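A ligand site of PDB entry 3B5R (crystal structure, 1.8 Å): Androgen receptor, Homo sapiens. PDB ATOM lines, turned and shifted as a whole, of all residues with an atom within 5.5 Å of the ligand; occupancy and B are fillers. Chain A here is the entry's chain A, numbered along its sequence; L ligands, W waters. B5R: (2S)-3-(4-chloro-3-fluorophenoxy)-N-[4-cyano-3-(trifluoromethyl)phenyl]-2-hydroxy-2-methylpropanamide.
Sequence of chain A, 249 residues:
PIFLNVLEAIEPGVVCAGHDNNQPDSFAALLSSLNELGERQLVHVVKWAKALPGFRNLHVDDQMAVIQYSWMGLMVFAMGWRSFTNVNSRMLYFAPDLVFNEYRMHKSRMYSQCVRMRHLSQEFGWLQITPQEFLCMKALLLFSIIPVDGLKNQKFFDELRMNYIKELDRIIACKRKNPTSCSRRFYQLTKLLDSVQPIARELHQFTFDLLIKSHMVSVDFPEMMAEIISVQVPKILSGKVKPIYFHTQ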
ATOM      1  N   LEU A  31      -0.733  20.275  21.840  1.00  0.00           N
ATOM      2  CA  LEU A  31      -0.577  20.037  23.267  1.00  0.00           C
ATOM      3  C   LEU A  31      -1.319  21.051  24.140  1.00  0.00           C
ATOM      4  O   LEU A  31      -1.881  20.697  25.170  1.00  0.00           O
ATOM      5  CB  LEU A  31       0.911  19.996  23.645  1.00  0.00           C
ATOM      6  CG  LEU A  31       1.435  18.573  23.839  1.00  0.00           C
ATOM      7  CD1 LEU A  31       0.725  17.951  25.046  1.00  0.00           C
ATOM      8  CD2 LEU A  31       1.190  17.726  22.576  1.00  0.00           C
ATOM      9  N   LEU A  34      -4.718  19.949  24.059  1.00  0.00           N
ATOM     10  CA  LEU A  34      -4.919  18.755  24.856  1.00  0.00           C
ATOM     11  C   LEU A  34      -4.973  19.168  26.320  1.00  0.00           C
ATOM     12  O   LEU A  34      -5.799  18.665  27.071  1.00  0.00           O
ATOM     13  CB  LEU A  34      -3.786  17.731  24.627  1.00  0.00           C
ATOM     14  CG  LEU A  34      -3.896  16.881  23.351  1.00  0.00           C
ATOM     15  CD1 LEU A  34      -2.690  15.946  23.215  1.00  0.00           C
ATOM     16  CD2 LEU A  34      -5.185  16.081  23.400  1.00  0.00           C
ATOM     17  N   ASN A  35      -4.115  20.107  26.718  1.00  0.00           N
ATOM     18  CA  ASN A  35      -4.109  20.572  28.098  1.00  0.00           C
ATOM     19  C   ASN A  35      -5.438  21.217  28.440  1.00  0.00           C
ATOM     20  O   ASN A  35      -6.046  20.886  29.459  1.00  0.00           O
ATOM     21  CB  ASN A  35      -2.976  21.580  28.344  1.00  0.00           C
ATOM     22  CG  ASN A  35      -1.609  20.944  28.392  1.00  0.00           C
ATOM     23  OD1 ASN A  35      -1.471  19.744  28.624  1.00  0.00           O
ATOM     24  ND2 ASN A  35      -0.561  21.748  28.185  1.00  0.00           N
ATOM     25  N   GLU A  36      -5.886  22.151  27.596  1.00  0.00           N
ATOM     26  CA  GLU A  36      -7.149  22.851  27.795  1.00  0.00           C
ATOM     27  C   GLU A  36      -8.314  21.861  27.828  1.00  0.00           C
ATOM     28  O   GLU A  36      -9.181  21.932  28.706  1.00  0.00           O
ATOM     29  CB  GLU A  36      -7.365  23.884  26.674  1.00  0.00           C
ATOM     30  CG  GLU A  36      -8.724  24.593  26.706  1.00  0.00           C
ATOM     31  CD  GLU A  36      -8.890  25.507  27.896  1.00  0.00           C
ATOM     32  OE1 GLU A  36     -10.037  25.924  28.170  1.00  0.00           O
ATOM     33  OE2 GLU A  36      -7.877  25.811  28.564  1.00  0.00           O
ATOM     34  N   LEU A  37      -8.340  20.923  26.875  1.00  0.00           N
ATOM     35  CA  LEU A  37      -9.408  19.923  26.837  1.00  0.00           C
ATOM     36  C   LEU A  37      -9.424  19.129  28.145  1.00  0.00           C
ATOM     37  O   LEU A  37     -10.477  18.931  28.738  1.00  0.00           O
ATOM     38  CB  LEU A  37      -9.231  18.971  25.661  1.00  0.00           C
ATOM     39  CG  LEU A  37     -10.267  17.849  25.538  1.00  0.00           C
ATOM     40  CD1 LEU A  37     -11.686  18.428  25.470  1.00  0.00           C
ATOM     41  CD2 LEU A  37      -9.973  17.028  24.295  1.00  0.00           C
ATOM     42  N   GLY A  38      -8.258  18.675  28.579  1.00  0.00           N
ATOM     43  CA  GLY A  38      -8.171  17.893  29.801  1.00  0.00           C
ATOM     44  C   GLY A  38      -8.773  18.636  30.972  1.00  0.00           C
ATOM     45  O   GLY A  38      -9.526  18.064  31.770  1.00  0.00           O
ATOM     46  N   GLN A  41     -12.610  18.834  30.702  1.00  0.00           N
ATOM     47  CA  GLN A  41     -13.241  17.561  31.068  1.00  0.00           C
ATOM     48  C   GLN A  41     -13.210  17.348  32.576  1.00  0.00           C
ATOM     49  O   GLN A  41     -14.116  16.730  33.135  1.00  0.00           O
ATOM     50  CB  GLN A  41     -12.566  16.390  30.326  1.00  0.00           C
ATOM     51  CG  GLN A  41     -12.819  16.436  28.820  1.00  0.00           C
ATOM     52  CD  GLN A  41     -12.388  15.184  28.088  1.00  0.00           C
ATOM     53  OE1 GLN A  41     -12.283  15.196  26.853  1.00  0.00           O
ATOM     54  NE2 GLN A  41     -12.149  14.090  28.814  1.00  0.00           N
ATOM     55  N   GLN A  68      -8.546  13.238  41.296  1.00  0.00           N
ATOM     56  CA  GLN A  68      -7.281  13.648  40.699  1.00  0.00           C
ATOM     57  C   GLN A  68      -6.416  12.475  40.233  1.00  0.00           C
ATOM     58  O   GLN A  68      -5.799  12.551  39.178  1.00  0.00           O
ATOM     59  CB  GLN A  68      -6.517  14.549  41.686  1.00  0.00           C
ATOM     60  CG  GLN A  68      -7.325  15.752  42.157  1.00  0.00           C
ATOM     61  CD  GLN A  68      -6.505  16.808  42.908  1.00  0.00           C
ATOM     62  OE1 GLN A  68      -5.490  16.493  43.528  1.00  0.00           O
ATOM     63  NE2 GLN A  68      -6.980  18.054  42.876  1.00  0.00           N
ATOM     64  N   TRP A  71      -8.359  10.788  37.222  1.00  0.00           N
ATOM     65  CA  TRP A  71      -8.611  11.717  36.125  1.00  0.00           C
ATOM     66  C   TRP A  71      -8.133  11.253  34.741  1.00  0.00           C
ATOM     67  O   TRP A  71      -8.936  11.180  33.792  1.00  0.00           O
ATOM     68  CB  TRP A  71      -7.979  13.073  36.503  1.00  0.00           C
ATOM     69  CG  TRP A  71      -8.127  14.187  35.505  1.00  0.00           C
ATOM     70  CD1 TRP A  71      -9.039  14.289  34.488  1.00  0.00           C
ATOM     71  CD2 TRP A  71      -7.354  15.394  35.455  1.00  0.00           C
ATOM     72  NE1 TRP A  71      -8.881  15.480  33.819  1.00  0.00           N
ATOM     73  CE2 TRP A  71      -7.855  16.183  34.394  1.00  0.00           C
ATOM     74  CE3 TRP A  71      -6.277  15.892  36.218  1.00  0.00           C
ATOM     75  CZ2 TRP A  71      -7.315  17.434  34.062  1.00  0.00           C
ATOM     76  CZ3 TRP A  71      -5.748  17.142  35.895  1.00  0.00           C
ATOM     77  CH2 TRP A  71      -6.277  17.896  34.832  1.00  0.00           C
ATOM     78  N   MET A  72      -6.859  10.913  34.605  1.00  0.00           N
ATOM     79  CA  MET A  72      -6.331  10.488  33.320  1.00  0.00           C
ATOM     80  C   MET A  72      -7.018   9.236  32.781  1.00  0.00           C
ATOM     81  O   MET A  72      -7.509   9.242  31.657  1.00  0.00           O
ATOM     82  CB  MET A  72      -4.825  10.223  33.410  1.00  0.00           C
ATOM     83  CG  MET A  72      -4.190   9.797  32.088  1.00  0.00           C
ATOM     84  SD  MET A  72      -4.267  11.092  30.861  1.00  0.00           S
ATOM     85  CE  MET A  72      -2.794  11.976  31.250  1.00  0.00           C
ATOM     86  N   MET A  75     -10.558   9.697  31.464  1.00  0.00           N
ATOM     87  CA  MET A  75     -10.613  10.363  30.179  1.00  0.00           C
ATOM     88  C   MET A  75     -10.232   9.386  29.068  1.00  0.00           C
ATOM     89  O   MET A  75     -10.844   9.380  27.996  1.00  0.00           O
ATOM     90  CB  MET A  75      -9.667  11.574  30.144  1.00  0.00           C
ATOM     91  CG  MET A  75     -10.042  12.696  31.093  1.00  0.00           C
ATOM     92  SD  MET A  75      -9.218  14.250  30.632  1.00  0.00           S
ATOM     93  CE  MET A  75      -7.563  13.915  31.173  1.00  0.00           C
ATOM     94  N   VAL A  76      -9.215   8.552  29.332  1.00  0.00           N
ATOM     95  CA  VAL A  76      -8.756   7.565  28.364  1.00  0.00           C
ATOM     96  C   VAL A  76      -9.881   6.595  28.004  1.00  0.00           C
ATOM     97  O   VAL A  76     -10.113   6.311  26.829  1.00  0.00           O
ATOM     98  CB  VAL A  76      -7.578   6.706  28.935  1.00  0.00           C
ATOM     99  CG1 VAL A  76      -7.349   5.503  28.041  1.00  0.00           C
ATOM    100  CG2 VAL A  76      -6.304   7.539  29.016  1.00  0.00           C
ATOM    101  N   MET A  79     -12.709   8.327  26.104  1.00  0.00           N
ATOM    102  CA  MET A  79     -12.227   8.709  24.779  1.00  0.00           C
ATOM    103  C   MET A  79     -12.222   7.496  23.850  1.00  0.00           C
ATOM    104  O   MET A  79     -12.639   7.599  22.697  1.00  0.00           O
ATOM    105  CB  MET A  79     -10.815   9.326  24.861  1.00  0.00           C
ATOM    106  CG  MET A  79     -10.326   9.984  23.558  1.00  0.00           C
ATOM    107  SD  MET A  79      -9.681   8.811  22.356  1.00  0.00           S
ATOM    108  CE  MET A  79      -7.936   8.754  22.808  1.00  0.00           C
ATOM    109  N   ARG A  82     -15.766   6.892  22.838  1.00  0.00           N
ATOM    110  CA  ARG A  82     -16.211   7.880  21.862  1.00  0.00           C
ATOM    111  C   ARG A  82     -15.585   7.590  20.507  1.00  0.00           C
ATOM    112  O   ARG A  82     -16.230   7.781  19.475  1.00  0.00           O
ATOM    113  CB  ARG A  82     -15.825   9.305  22.283  1.00  0.00           C
ATOM    114  CG  ARG A  82     -16.727   9.939  23.325  1.00  0.00           C
ATOM    115  CD  ARG A  82     -16.496  11.450  23.403  1.00  0.00           C
ATOM    116  NE  ARG A  82     -15.084  11.774  23.563  1.00  0.00           N
ATOM    117  CZ  ARG A  82     -14.432  11.760  24.718  1.00  0.00           C
ATOM    118  NH1 ARG A  82     -15.063  11.459  25.844  1.00  0.00           N
ATOM    119  NH2 ARG A  82     -13.139  12.046  24.749  1.00  0.00           N
ATOM    120  N   TYR A  93     -11.085  10.143  18.879  1.00  0.00           N
ATOM    121  CA  TYR A  93     -12.058  11.222  19.060  1.00  0.00           C
ATOM    122  C   TYR A  93     -11.882  11.898  20.430  1.00  0.00           C
ATOM    123  O   TYR A  93     -12.697  11.699  21.336  1.00  0.00           O
ATOM    124  CB  TYR A  93     -13.460  10.635  18.935  1.00  0.00           C
ATOM    125  CG  TYR A  93     -14.551  11.596  18.555  1.00  0.00           C
ATOM    126  CD1 TYR A  93     -14.800  11.914  17.215  1.00  0.00           C
ATOM    127  CD2 TYR A  93     -15.377  12.172  19.522  1.00  0.00           C
ATOM    128  CE1 TYR A  93     -15.844  12.769  16.848  1.00  0.00           C
ATOM    129  CE2 TYR A  93     -16.423  13.022  19.174  1.00  0.00           C
ATOM    130  CZ  TYR A  93     -16.648  13.313  17.842  1.00  0.00           C
ATOM    131  OH  TYR A  93     -17.677  14.156  17.506  1.00  0.00           O
ATOM    132  N   PHE A  94     -10.828  12.692  20.585  1.00  0.00           N
ATOM    133  CA  PHE A  94     -10.609  13.377  21.849  1.00  0.00           C
ATOM    134  C   PHE A  94     -11.786  14.306  22.112  1.00  0.00           C
ATOM    135  O   PHE A  94     -12.301  14.394  23.229  1.00  0.00           O
ATOM    136  CB  PHE A  94      -9.319  14.185  21.812  1.00  0.00           C
ATOM    137  CG  PHE A  94      -8.068  13.348  21.871  1.00  0.00           C
ATOM    138  CD1 PHE A  94      -7.386  13.020  20.702  1.00  0.00           C
ATOM    139  CD2 PHE A  94      -7.565  12.917  23.086  1.00  0.00           C
ATOM    140  CE1 PHE A  94      -6.207  12.280  20.762  1.00  0.00           C
ATOM    141  CE2 PHE A  94      -6.377  12.174  23.157  1.00  0.00           C
ATOM    142  CZ  PHE A  94      -5.702  11.857  21.989  1.00  0.00           C
ATOM    143  N   MET A 110       3.025  11.759  21.173  1.00  0.00           N
ATOM    144  CA  MET A 110       2.392  10.798  22.086  1.00  0.00           C
ATOM    145  C   MET A 110       1.921   9.612  21.251  1.00  0.00           C
ATOM    146  O   MET A 110       0.888   9.010  21.558  1.00  0.00           O
ATOM    147  CB  MET A 110       1.161  11.416  22.746  1.00  0.00           C
ATOM    148  CG  MET A 110       1.364  12.785  23.357  1.00  0.00           C
ATOM    149  SD  MET A 110      -0.211  13.414  23.992  1.00  0.00           S
ATOM    150  CE  MET A 110      -0.310  12.556  25.490  1.00  0.00           C
ATOM    151  N   MET A 117      -4.385   3.469  22.808  1.00  0.00           N
ATOM    152  CA  MET A 117      -5.775   3.882  23.037  1.00  0.00           C
ATOM    153  C   MET A 117      -6.659   3.521  21.835  1.00  0.00           C
ATOM    154  O   MET A 117      -7.865   3.323  21.971  1.00  0.00           O
ATOM    155  CB  MET A 117      -5.832   5.386  23.320  1.00  0.00           C
ATOM    156  CG  MET A 117      -5.109   5.791  24.592  1.00  0.00           C
ATOM    157  SD  MET A 117      -5.380   7.497  25.109  1.00  0.00           S
ATOM    158  CE  MET A 117      -4.269   8.359  24.013  1.00  0.00           C
ATOM    159  N   LEU A 203       0.869   8.165  29.842  1.00  0.00           N
ATOM    160  CA  LEU A 203       0.462   9.550  29.625  1.00  0.00           C
ATOM    161  C   LEU A 203       0.909  10.398  30.814  1.00  0.00           C
ATOM    162  O   LEU A 203       1.332  11.557  30.641  1.00  0.00           O
ATOM    163  CB  LEU A 203      -1.066   9.624  29.436  1.00  0.00           C
ATOM    164  CG  LEU A 203      -1.610   9.035  28.127  1.00  0.00           C
ATOM    165  CD1 LEU A 203      -3.123   9.031  28.150  1.00  0.00           C
ATOM    166  CD2 LEU A 203      -1.110   9.832  26.930  1.00  0.00           C
ATOM    167  N   HIS A 204       0.819   9.827  32.006  1.00  0.00           N
ATOM    168  CA  HIS A 204       1.254  10.536  33.213  1.00  0.00           C
ATOM    169  C   HIS A 204       2.745  10.858  33.074  1.00  0.00           C
ATOM    170  O   HIS A 204       3.156  12.007  33.239  1.00  0.00           O
ATOM    171  CB  HIS A 204       1.039   9.652  34.451  1.00  0.00           C
ATOM    172  CG  HIS A 204      -0.328   9.750  35.026  1.00  0.00           C
ATOM    173  ND1 HIS A 204      -0.938   8.693  35.682  1.00  0.00           N
ATOM    174  CD2 HIS A 204      -1.218  10.774  35.072  1.00  0.00           C
ATOM    175  CE1 HIS A 204      -2.128   9.069  36.107  1.00  0.00           C
ATOM    176  NE2 HIS A 204      -2.324  10.324  35.744  1.00  0.00           N
ATOM    177  N   PHE A 206       4.651  10.937  30.410  1.00  0.00           N
ATOM    178  CA  PHE A 206       4.854  11.880  29.319  1.00  0.00           C
ATOM    179  C   PHE A 206       4.542  13.313  29.747  1.00  0.00           C
ATOM    180  O   PHE A 206       5.355  14.216  29.540  1.00  0.00           O
ATOM    181  CB  PHE A 206       3.988  11.499  28.104  1.00  0.00           C
ATOM    182  CG  PHE A 206       3.818  12.601  27.089  1.00  0.00           C
ATOM    183  CD1 PHE A 206       2.788  13.536  27.219  1.00  0.00           C
ATOM    184  CD2 PHE A 206       4.683  12.719  26.007  1.00  0.00           C
ATOM    185  CE1 PHE A 206       2.626  14.564  26.282  1.00  0.00           C
ATOM    186  CE2 PHE A 206       4.530  13.738  25.058  1.00  0.00           C
ATOM    187  CZ  PHE A 206       3.497  14.661  25.195  1.00  0.00           C
ATOM    188  N   THR A 207       3.379  13.511  30.352  1.00  0.00           N
ATOM    189  CA  THR A 207       2.985  14.845  30.777  1.00  0.00           C
ATOM    190  C   THR A 207       3.914  15.402  31.833  1.00  0.00           C
ATOM    191  O   THR A 207       4.227  16.600  31.840  1.00  0.00           O
ATOM    192  CB  THR A 207       1.551  14.867  31.335  1.00  0.00           C
ATOM    193  OG1 THR A 207       0.665  14.199  30.435  1.00  0.00           O
ATOM    194  CG2 THR A 207       1.072  16.317  31.494  1.00  0.00           C
ATOM    195  N   PHE A 208       4.362  14.545  32.746  1.00  0.00           N
ATOM    196  CA  PHE A 208       5.271  14.997  33.775  1.00  0.00           C
ATOM    197  C   PHE A 208       6.565  15.525  33.147  1.00  0.00           C
ATOM    198  O   PHE A 208       7.003  16.623  33.450  1.00  0.00           O
ATOM    199  CB  PHE A 208       5.624  13.863  34.736  1.00  0.00           C
ATOM    200  CG  PHE A 208       6.700  14.218  35.726  1.00  0.00           C
ATOM    201  CD1 PHE A 208       6.410  14.962  36.859  1.00  0.00           C
ATOM    202  CD2 PHE A 208       8.021  13.819  35.501  1.00  0.00           C
ATOM    203  CE1 PHE A 208       7.417  15.299  37.772  1.00  0.00           C
ATOM    204  CE2 PHE A 208       9.038  14.146  36.403  1.00  0.00           C
ATOM    205  CZ  PHE A 208       8.736  14.889  37.544  1.00  0.00           C
ATOM    206  N   PHE A 221       0.564  25.296  30.211  1.00  0.00           N
ATOM    207  CA  PHE A 221      -0.094  24.437  31.195  1.00  0.00           C
ATOM    208  C   PHE A 221      -1.051  25.220  32.067  1.00  0.00           C
ATOM    209  O   PHE A 221      -0.659  26.168  32.743  1.00  0.00           O
ATOM    210  CB  PHE A 221       0.918  23.700  32.071  1.00  0.00           C
ATOM    211  CG  PHE A 221       1.423  22.422  31.468  1.00  0.00           C
ATOM    212  CD1 PHE A 221       2.605  22.398  30.739  1.00  0.00           C
ATOM    213  CD2 PHE A 221       0.693  21.250  31.594  1.00  0.00           C
ATOM    214  CE1 PHE A 221       3.052  21.227  30.131  1.00  0.00           C
ATOM    215  CE2 PHE A 221       1.127  20.069  30.992  1.00  0.00           C
ATOM    216  CZ  PHE A 221       2.309  20.046  30.264  1.00  0.00           C
ATOM    217  N   MET A 225      -4.097  22.036  36.283  1.00  0.00           N
ATOM    218  CA  MET A 225      -3.353  20.892  35.754  1.00  0.00           C
ATOM    219  C   MET A 225      -1.910  20.883  36.246  1.00  0.00           C
ATOM    220  O   MET A 225      -1.429  19.856  36.732  1.00  0.00           O
ATOM    221  CB  MET A 225      -3.380  20.879  34.225  1.00  0.00           C
ATOM    222  CG  MET A 225      -2.851  19.572  33.629  1.00  0.00           C
ATOM    223  SD  MET A 225      -2.912  19.478  31.828  1.00  0.00           S
ATOM    224  CE  MET A 225      -4.682  19.131  31.581  1.00  0.00           C
ATOM    225  N   ILE A 228      -1.794  19.772  39.840  1.00  0.00           N
ATOM    226  CA  ILE A 228      -2.076  18.352  39.983  1.00  0.00           C
ATOM    227  C   ILE A 228      -0.917  17.481  39.503  1.00  0.00           C
ATOM    228  O   ILE A 228      -0.576  16.487  40.132  1.00  0.00           O
ATOM    229  CB  ILE A 228      -3.365  17.974  39.239  1.00  0.00           C
ATOM    230  CG1 ILE A 228      -4.561  18.627  39.943  1.00  0.00           C
ATOM    231  CG2 ILE A 228      -3.526  16.458  39.170  1.00  0.00           C
ATOM    232  CD1 ILE A 228      -5.890  18.452  39.218  1.00  0.00           C
ATOM    233  N   ILE A 229      -0.310  17.860  38.381  1.00  0.00           N
ATOM    234  CA  ILE A 229       0.814  17.124  37.813  1.00  0.00           C
ATOM    235  C   ILE A 229       2.045  17.158  38.710  1.00  0.00           C
ATOM    236  O   ILE A 229       2.778  16.176  38.786  1.00  0.00           O
ATOM    237  CB  ILE A 229       1.228  17.689  36.438  1.00  0.00           C
ATOM    238  CG1 ILE A 229       0.064  17.549  35.454  1.00  0.00           C
ATOM    239  CG2 ILE A 229       2.463  16.969  35.930  1.00  0.00           C
ATOM    240  CD1 ILE A 229       0.346  18.175  34.104  1.00  0.00           C
ATOM    241  N   VAL A 233       0.584  13.492  40.400  1.00  0.00           N
ATOM    242  CA  VAL A 233       1.227  12.564  39.471  1.00  0.00           C
ATOM    243  C   VAL A 233       2.559  12.013  39.990  1.00  0.00           C
ATOM    244  O   VAL A 233       2.854  10.832  39.782  1.00  0.00           O
ATOM    245  CB  VAL A 233       1.458  13.236  38.104  1.00  0.00           C
ATOM    246  CG1 VAL A 233       2.234  12.304  37.173  1.00  0.00           C
ATOM    247  CG2 VAL A 233       0.117  13.570  37.494  1.00  0.00           C
HETATM  248  C21 B5R L   1      -1.889  14.814  32.523  1.00  0.00           C
HETATM  249  C20 B5R L   1      -1.897  14.500  33.880  1.00  0.00           C
HETATM  250  F20 B5R L   1      -0.712  14.245  34.465  1.00  0.00           F
HETATM  251  C19 B5R L   1      -3.103  14.444  34.566  1.00  0.00           C
HETATM  252 CL19 B5R L   1      -3.199  14.002  36.243  1.00  0.00          CL
HETATM  253  C18 B5R L   1      -4.295  14.731  33.904  1.00  0.00           C
HETATM  254  C17 B5R L   1      -4.287  15.045  32.547  1.00  0.00           C
HETATM  255  C16 B5R L   1      -3.085  15.082  31.856  1.00  0.00           C
HETATM  256  O14 B5R L   1      -3.074  15.174  30.502  1.00  0.00           O
HETATM  257  C13 B5R L   1      -2.891  16.506  30.003  1.00  0.00           C
HETATM  258  C11 B5R L   1      -2.751  16.372  28.491  1.00  0.00           C
HETATM  259  O11 B5R L   1      -3.112  17.616  27.885  1.00  0.00           O
HETATM  260  C12 B5R L   1      -1.309  16.003  28.135  1.00  0.00           C
HETATM  261  C10 B5R L   1      -3.710  15.271  28.021  1.00  0.00           C
HETATM  262  O10 B5R L   1      -3.339  14.108  27.932  1.00  0.00           O
HETATM  263  N9  B5R L   1      -4.950  15.702  27.778  1.00  0.00           N
HETATM  264  C6  B5R L   1      -5.971  14.953  27.380  1.00  0.00           C
HETATM  265  C5  B5R L   1      -5.913  13.567  27.248  1.00  0.00           C
HETATM  266  C1  B5R L   1      -7.189  15.599  27.179  1.00  0.00           C
HETATM  267  C2  B5R L   1      -8.320  14.852  26.859  1.00  0.00           C
HETATM  268  C3  B5R L   1      -8.241  13.469  26.741  1.00  0.00           C
HETATM  269  C8  B5R L   1      -9.467  12.797  26.403  1.00  0.00           C
HETATM  270  N8  B5R L   1     -10.440  12.278  26.137  1.00  0.00           N
HETATM  271  C4  B5R L   1      -7.039  12.796  26.933  1.00  0.00           C
HETATM  272  C7  B5R L   1      -6.918  11.263  26.880  1.00  0.00           C
HETATM  273  F2  B5R L   1      -7.626  10.710  25.887  1.00  0.00           F
HETATM  274  F1  B5R L   1      -5.674  10.850  26.682  1.00  0.00           F
HETATM  275  F3  B5R L   1      -7.345  10.728  28.023  1.00  0.00           F
HETATM  276  O   HOH W   1     -12.723  11.551  28.008  1.00  0.00           O
HETATM  277  O   HOH W   2      -4.818  11.076  36.722  1.00  0.00           O
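O of Leu 34 sits close to O11 of the ligand, 3.0 Å away.
A nitrogen (N8) of the ligand is in hydrogen-bond range of the guanidinium group (NH2) of Arg 82 (3.0 Å).
O11 of the ligand lies within hydrogen-bond range of N of Asn 35, at 2.9 Å.
The side-chain amide oxygen of Asn 35 sits at hydrogen-bond distance from an oxygen (O11) of the ligand.
The guanidinium group of Arg 82 lies within hydrogen-bond range of the backbone carbonyl oxygen of Tyr 93.
The side-chain amide nitrogen of Asn 35 sits close to the backbone carbonyl oxygen of Leu 31 (3.5 Å).
The backbone carbonyl oxygen of Leu 203 sits at hydrogen-bond distance from the side-chain hydroxyl of Thr 207, 2.7 Å away.
O of Gly 38 sits close to NE1 of Trp 71.
The side-chain sulfur (SD) of Met 75 sits close to the indole nitrogen (NE1) of Trp 71 (3.4 Å).
The backbone NH of Val 233 lies within hydrogen-bond range of the backbone carbonyl oxygen of Ile 228 (3.2 Å).
The side-chain amide oxygen (OD1) of Asn 35 sits close to the side-chain sulfur (SD) of Met 225, at 3.5 Å.
The guanidinium group (NH2) of Arg 82 lies within hydrogen-bond range of the backbone carbonyl oxygen (O) of Phe 94 (2.9 Å).
The backbone carbonyl oxygen (O) of Met 75 sits close to a nitrogen (N8) of the ligand (3.5 Å).
N of Val 76 lies close to F3 of the ligand, 3.2 Å away.
The side-chain sulfur (SD) of Met 117 sits close to a fluorine (F1) of the ligand (3.7 Å).
Leu 37 touches the ligand.
Gly 38 touches the ligand (N to C1, 3.5 Å).
Gln 41 touches the ligand.
Trp 71 touches the ligand.
Met 72 touches the ligand (CE to C16, 3.2 Å).
CB of Met 79 touches N8 of the ligand (3.2 Å).
Phe 94 touches the ligand (CE2 to F2, 3.3 Å).
Leu 203 touches the ligand (CD1 to F1, 3.5 Å).
CD2 of His 204 touches F20 of the ligand, at 3.6 Å.
Thr 207 touches the ligand (OG1 to C21, 3.4 Å).
Met 225 touches the ligand (SD to C13, 3.5 Å).
Ile 228 touches the ligand (CG2 to CL19, 3.8 Å).
CG1 of Ile 229 touches F20 of the ligand, at 3.5 Å.
Val 233 touches the ligand.
Hydrophobic or aromatic side chains that line the ligand: Leu 34, Leu 37, Trp 71, Met 72, Met 75, Val 76, Met 79, Phe 94, Met 117, Leu 203, His 204, Met 225, Ile 228, Ile 229 and Val 233.
Of the 28 residues printed, 20 come within 4 Å of the ligand.
The nearest printed residue that does not touch the ligand is Leu 31 (4.2 Å).
Water W1 lies within hydrogen-bond range of the side-chain amide nitrogen of Gln 41, the backbone carbonyl oxygen of Met 75, a nitrogen (N8) of the ligand and the guanidinium group of Arg 82.
Water W2 lies within hydrogen-bond range of a ring nitrogen (NE2) of His 204 (2.8 Å), the backbone NH of Met 72 (2.9 Å) and the backbone carbonyl oxygen of Gln 68 (3.0 Å).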
